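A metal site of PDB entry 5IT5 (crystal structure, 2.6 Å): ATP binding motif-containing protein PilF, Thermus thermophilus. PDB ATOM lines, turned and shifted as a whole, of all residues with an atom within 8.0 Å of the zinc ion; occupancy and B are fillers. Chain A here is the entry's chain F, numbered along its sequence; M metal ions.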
ATOM      1  N   VAL A 276     -23.094  10.160  -7.769  1.00  0.00           N
ATOM      2  CA  VAL A 276     -21.876   9.379  -8.058  1.00  0.00           C
ATOM      3  C   VAL A 276     -21.826   8.051  -7.325  1.00  0.00           C
ATOM      4  O   VAL A 276     -21.938   7.996  -6.096  1.00  0.00           O
ATOM      5  CB  VAL A 276     -20.612  10.156  -7.710  1.00  0.00           C
ATOM      6  CG1 VAL A 276     -19.399   9.274  -7.880  1.00  0.00           C
ATOM      7  CG2 VAL A 276     -20.498  11.394  -8.582  1.00  0.00           C
ATOM      8  N   CYS A 277     -21.653   6.967  -8.077  1.00  0.00           N
ATOM      9  CA  CYS A 277     -21.520   5.630  -7.505  1.00  0.00           C
ATOM     10  C   CYS A 277     -20.383   5.575  -6.482  1.00  0.00           C
ATOM     11  O   CYS A 277     -19.245   5.975  -6.752  1.00  0.00           O
ATOM     12  CB  CYS A 277     -21.321   4.589  -8.617  1.00  0.00           C
ATOM     13  SG  CYS A 277     -20.885   2.914  -8.076  1.00  0.00           S
ATOM     14  N   GLU A 278     -20.714   5.083  -5.293  1.00  0.00           N
ATOM     15  CA  GLU A 278     -19.739   4.998  -4.211  1.00  0.00           C
ATOM     16  C   GLU A 278     -18.580   4.031  -4.506  1.00  0.00           C
ATOM     17  O   GLU A 278     -17.436   4.313  -4.159  1.00  0.00           O
ATOM     18  CB  GLU A 278     -20.438   4.589  -2.929  1.00  0.00           C
ATOM     19  CG  GLU A 278     -20.021   5.431  -1.784  1.00  0.00           C
ATOM     20  CD  GLU A 278     -20.357   6.882  -2.004  1.00  0.00           C
ATOM     21  OE1 GLU A 278     -21.557   7.206  -1.961  1.00  0.00           O
ATOM     22  OE2 GLU A 278     -19.425   7.694  -2.241  1.00  0.00           O
ATOM     23  N   HIS A 279     -18.899   2.916  -5.162  1.00  0.00           N
ATOM     24  CA  HIS A 279     -17.935   1.860  -5.426  1.00  0.00           C
ATOM     25  C   HIS A 279     -16.831   2.287  -6.379  1.00  0.00           C
ATOM     26  O   HIS A 279     -15.698   1.846  -6.241  1.00  0.00           O
ATOM     27  CB  HIS A 279     -18.618   0.605  -5.979  1.00  0.00           C
ATOM     28  CG  HIS A 279     -17.887  -0.666  -5.638  1.00  0.00           C
ATOM     29  ND1 HIS A 279     -17.135  -0.805  -4.488  1.00  0.00           N
ATOM     30  CD2 HIS A 279     -17.784  -1.844  -6.306  1.00  0.00           C
ATOM     31  CE1 HIS A 279     -16.601  -2.016  -4.452  1.00  0.00           C
ATOM     32  NE2 HIS A 279     -16.987  -2.663  -5.538  1.00  0.00           N
ATOM     33  N   CYS A 280     -17.144   3.163  -7.331  1.00  0.00           N
ATOM     34  CA  CYS A 280     -16.100   3.586  -8.257  1.00  0.00           C
ATOM     35  C   CYS A 280     -15.814   5.080  -8.237  1.00  0.00           C
ATOM     36  O   CYS A 280     -15.236   5.595  -9.201  1.00  0.00           O
ATOM     37  CB  CYS A 280     -16.448   3.169  -9.687  1.00  0.00           C
ATOM     38  SG  CYS A 280     -18.114   3.524 -10.251  1.00  0.00           S
ATOM     39  N   LYS A 281     -16.206   5.760  -7.154  1.00  0.00           N
ATOM     40  CA  LYS A 281     -15.892   7.186  -6.947  1.00  0.00           C
ATOM     41  C   LYS A 281     -14.371   7.330  -7.018  1.00  0.00           C
ATOM     42  O   LYS A 281     -13.637   6.512  -6.489  1.00  0.00           O
ATOM     43  CB  LYS A 281     -16.427   7.680  -5.606  1.00  0.00           C
ATOM     44  CG  LYS A 281     -16.554   9.191  -5.378  1.00  0.00           C
ATOM     45  CD  LYS A 281     -16.816   9.414  -3.891  1.00  0.00           C
ATOM     46  CE  LYS A 281     -17.802  10.524  -3.581  1.00  0.00           C
ATOM     47  NZ  LYS A 281     -19.174   9.995  -3.724  1.00  0.00           N
ATOM     48  N   LYS A 308     -15.846  11.671  -9.622  1.00  0.00           N
ATOM     49  CA  LYS A 308     -16.427  11.002 -10.781  1.00  0.00           C
ATOM     50  C   LYS A 308     -16.578   9.499 -10.538  1.00  0.00           C
ATOM     51  O   LYS A 308     -15.733   8.884  -9.899  1.00  0.00           O
ATOM     52  CB  LYS A 308     -15.534  11.229 -12.020  1.00  0.00           C
ATOM     53  CG  LYS A 308     -15.659  10.171 -13.100  1.00  0.00           C
ATOM     54  CD  LYS A 308     -14.293   9.711 -13.648  1.00  0.00           C
ATOM     55  CE  LYS A 308     -13.536  10.824 -14.328  1.00  0.00           C
ATOM     56  NZ  LYS A 308     -12.575  10.266 -15.326  1.00  0.00           N
ATOM     57  N   GLY A 309     -17.649   8.917 -11.041  1.00  0.00           N
ATOM     58  CA  GLY A 309     -17.780   7.467 -11.117  1.00  0.00           C
ATOM     59  C   GLY A 309     -17.114   6.891 -12.364  1.00  0.00           C
ATOM     60  O   GLY A 309     -17.327   7.360 -13.495  1.00  0.00           O
ATOM     61  N   MET A 310     -16.324   5.854 -12.162  1.00  0.00           N
ATOM     62  CA  MET A 310     -15.572   5.212 -13.228  1.00  0.00           C
ATOM     63  C   MET A 310     -16.437   4.339 -14.072  1.00  0.00           C
ATOM     64  O   MET A 310     -16.264   4.277 -15.280  1.00  0.00           O
ATOM     65  CB  MET A 310     -14.450   4.367 -12.642  1.00  0.00           C
ATOM     66  CG  MET A 310     -13.349   5.195 -12.113  1.00  0.00           C
ATOM     67  SD  MET A 310     -12.218   5.539 -13.447  1.00  0.00           S
ATOM     68  CE  MET A 310     -11.388   6.942 -12.767  1.00  0.00           C
ATOM     69  N   GLY A 311     -17.373   3.673 -13.409  1.00  0.00           N
ATOM     70  CA  GLY A 311     -18.204   2.671 -14.051  1.00  0.00           C
ATOM     71  C   GLY A 311     -17.863   1.281 -13.545  1.00  0.00           C
ATOM     72  O   GLY A 311     -16.688   0.899 -13.544  1.00  0.00           O
ATOM     73  N   CYS A 312     -18.869   0.515 -13.103  1.00  0.00           N
ATOM     74  CA  CYS A 312     -18.619  -0.815 -12.563  1.00  0.00           C
ATOM     75  C   CYS A 312     -19.892  -1.638 -12.623  1.00  0.00           C
ATOM     76  O   CYS A 312     -20.948  -1.117 -12.975  1.00  0.00           O
ATOM     77  CB  CYS A 312     -18.077  -0.727 -11.131  1.00  0.00           C
ATOM     78  SG  CYS A 312     -19.247  -0.144  -9.880  1.00  0.00           S
ATOM     79  N   GLU A 313     -19.814  -2.931 -12.302  1.00  0.00           N
ATOM     80  CA  GLU A 313     -20.977  -3.762 -12.566  1.00  0.00           C
ATOM     81  C   GLU A 313     -22.018  -3.305 -11.476  1.00  0.00           C
ATOM     82  O   GLU A 313     -23.200  -3.622 -11.586  1.00  0.00           O
ATOM     83  CB  GLU A 313     -20.575  -5.258 -12.623  1.00  0.00           C
ATOM     84  CG  GLU A 313     -21.642  -6.257 -12.760  1.00  0.00           C
ATOM     85  CD  GLU A 313     -22.432  -6.491 -11.456  1.00  0.00           C
ATOM     86  OE1 GLU A 313     -21.970  -6.291 -10.359  1.00  0.00           O
ATOM     87  OE2 GLU A 313     -23.597  -6.891 -11.632  1.00  0.00           O
ATOM     88  N   ARG A 314     -21.660  -2.397 -10.556  1.00  0.00           N
ATOM     89  CA  ARG A 314     -22.631  -1.974  -9.526  1.00  0.00           C
ATOM     90  C   ARG A 314     -23.589  -0.926 -10.066  1.00  0.00           C
ATOM     91  O   ARG A 314     -24.770  -0.916  -9.748  1.00  0.00           O
ATOM     92  CB  ARG A 314     -21.920  -1.468  -8.269  1.00  0.00           C
ATOM     93  CG  ARG A 314     -22.318  -2.260  -7.035  1.00  0.00           C
ATOM     94  CD  ARG A 314     -21.132  -2.896  -6.366  1.00  0.00           C
ATOM     95  NE  ARG A 314     -21.314  -2.979  -4.906  1.00  0.00           N
ATOM     96  CZ  ARG A 314     -20.436  -3.505  -4.062  1.00  0.00           C
ATOM     97  NH1 ARG A 314     -19.298  -4.054  -4.505  1.00  0.00           N
ATOM     98  NH2 ARG A 314     -20.690  -3.509  -2.768  1.00  0.00           N
ATOM     99  N   CYS A 315     -23.064  -0.079 -10.939  1.00  0.00           N
ATOM    100  CA  CYS A 315     -23.804   1.014 -11.547  1.00  0.00           C
ATOM    101  C   CYS A 315     -23.948   0.907 -13.080  1.00  0.00           C
ATOM    102  O   CYS A 315     -24.141   1.921 -13.770  1.00  0.00           O
ATOM    103  CB  CYS A 315     -23.112   2.318 -11.192  1.00  0.00           C
ATOM    104  SG  CYS A 315     -21.443   2.451 -11.892  1.00  0.00           S
ATOM    105  N   GLY A 316     -23.843  -0.296 -13.628  1.00  0.00           N
ATOM    106  CA  GLY A 316     -24.045  -0.472 -15.053  1.00  0.00           C
ATOM    107  C   GLY A 316     -23.059   0.309 -15.894  1.00  0.00           C
ATOM    108  O   GLY A 316     -23.350   0.638 -17.039  1.00  0.00           O
ATOM    109  N   GLY A 317     -21.902   0.644 -15.346  1.00  0.00           N
ATOM    110  CA  GLY A 317     -20.895   1.405 -16.093  1.00  0.00           C
ATOM    111  C   GLY A 317     -21.259   2.875 -16.228  1.00  0.00           C
ATOM    112  O   GLY A 317     -20.596   3.628 -16.922  1.00  0.00           O
ATOM    113  N   THR A 318     -22.326   3.271 -15.561  1.00  0.00           N
ATOM    114  CA  THR A 318     -22.821   4.633 -15.594  1.00  0.00           C
ATOM    115  C   THR A 318     -21.908   5.577 -14.819  1.00  0.00           C
ATOM    116  O   THR A 318     -21.674   6.727 -15.226  1.00  0.00           O
ATOM    117  CB  THR A 318     -24.227   4.696 -14.991  1.00  0.00           C
ATOM    118  OG1 THR A 318     -25.092   3.812 -15.719  1.00  0.00           O
ATOM    119  CG2 THR A 318     -24.779   6.082 -15.059  1.00  0.00           C
ATOM    120  N   GLY A 319     -21.399   5.059 -13.699  1.00  0.00           N
ATOM    121  CA  GLY A 319     -20.654   5.837 -12.715  1.00  0.00           C
ATOM    122  C   GLY A 319     -21.605   6.606 -11.821  1.00  0.00           C
ATOM    123  O   GLY A 319     -21.183   7.508 -11.094  1.00  0.00           O
ATOM    124  N   TYR A 320     -22.897   6.279 -11.894  1.00  0.00           N
ATOM    125  CA  TYR A 320     -23.924   6.891 -11.076  1.00  0.00           C
ATOM    126  C   TYR A 320     -24.865   5.846 -10.503  1.00  0.00           C
ATOM    127  O   TYR A 320     -25.118   4.805 -11.128  1.00  0.00           O
ATOM    128  CB  TYR A 320     -24.761   7.884 -11.863  1.00  0.00           C
ATOM    129  CG  TYR A 320     -24.008   9.059 -12.455  1.00  0.00           C
ATOM    130  CD1 TYR A 320     -23.528  10.069 -11.628  1.00  0.00           C
ATOM    131  CD2 TYR A 320     -23.804   9.169 -13.840  1.00  0.00           C
ATOM    132  CE1 TYR A 320     -22.847  11.164 -12.161  1.00  0.00           C
ATOM    133  CE2 TYR A 320     -23.131  10.259 -14.388  1.00  0.00           C
ATOM    134  CZ  TYR A 320     -22.650  11.254 -13.535  1.00  0.00           C
ATOM    135  OH  TYR A 320     -21.974  12.345 -14.001  1.00  0.00           O
ATOM    136  N   LYS A 321     -25.387   6.128  -9.309  1.00  0.00           N
ATOM    137  CA  LYS A 321     -26.375   5.276  -8.683  1.00  0.00           C
ATOM    138  C   LYS A 321     -27.255   6.108  -7.776  1.00  0.00           C
ATOM    139  O   LYS A 321     -26.808   6.588  -6.740  1.00  0.00           O
ATOM    140  CB  LYS A 321     -25.726   4.158  -7.888  1.00  0.00           C
ATOM    141  CG  LYS A 321     -26.729   3.305  -7.155  1.00  0.00           C
ATOM    142  CD  LYS A 321     -26.473   1.839  -7.395  1.00  0.00           C
ATOM    143  CE  LYS A 321     -25.872   1.235  -6.165  1.00  0.00           C
ATOM    144  NZ  LYS A 321     -26.916   1.202  -5.109  1.00  0.00           N
HETATM  145 ZN    ZN M   1     -19.904   2.086 -10.116  1.00  0.00          ZN
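The side-chain sulfur (SG) of Cys 280 lies close to the backbone NH (N) of Gly 311, at 3.2 Å. The backbone carbonyl oxygen (O) of Cys 280 is in hydrogen-bond range of the backbone NH (N) of Met 310, at 3.2 Å. N of Arg 314 sits close to SG of Cys 312 (3.4 Å). The backbone carbonyl oxygen (O) of Cys 312 is in hydrogen-bond range of the backbone NH (N) of Gly 317, at 3.1 Å. SG of Cys 315 sits close to N of Gly 319 (3.2 Å). The side-chain hydroxyl (OG1) of Thr 318 is in hydrogen-bond range of the backbone carbonyl oxygen (O) of Cys 315 (2.9 Å). The backbone NH (N) of His 279 sits close to the side-chain sulfur (SG) of Cys 277 (3.5 Å). N of Cys 277 lies within hydrogen-bond range of O of Gly 319.
Within 4 Å of the zinc ion: Cys 277, Cys 280, Cys 312 and Cys 315. The nearest printed residue that does not touch the zinc ion is Gly 311 (4.1 Å).
The zinc ion is bound by the side-chain sulfur (SG) of Cys 280 (2.3 Å), the side-chain sulfur (SG) of Cys 312 (2.3 Å), the side-chain sulfur (SG) of Cys 315 (2.4 Å) and the side-chain sulfur (SG) of Cys 277 (2.4 Å).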
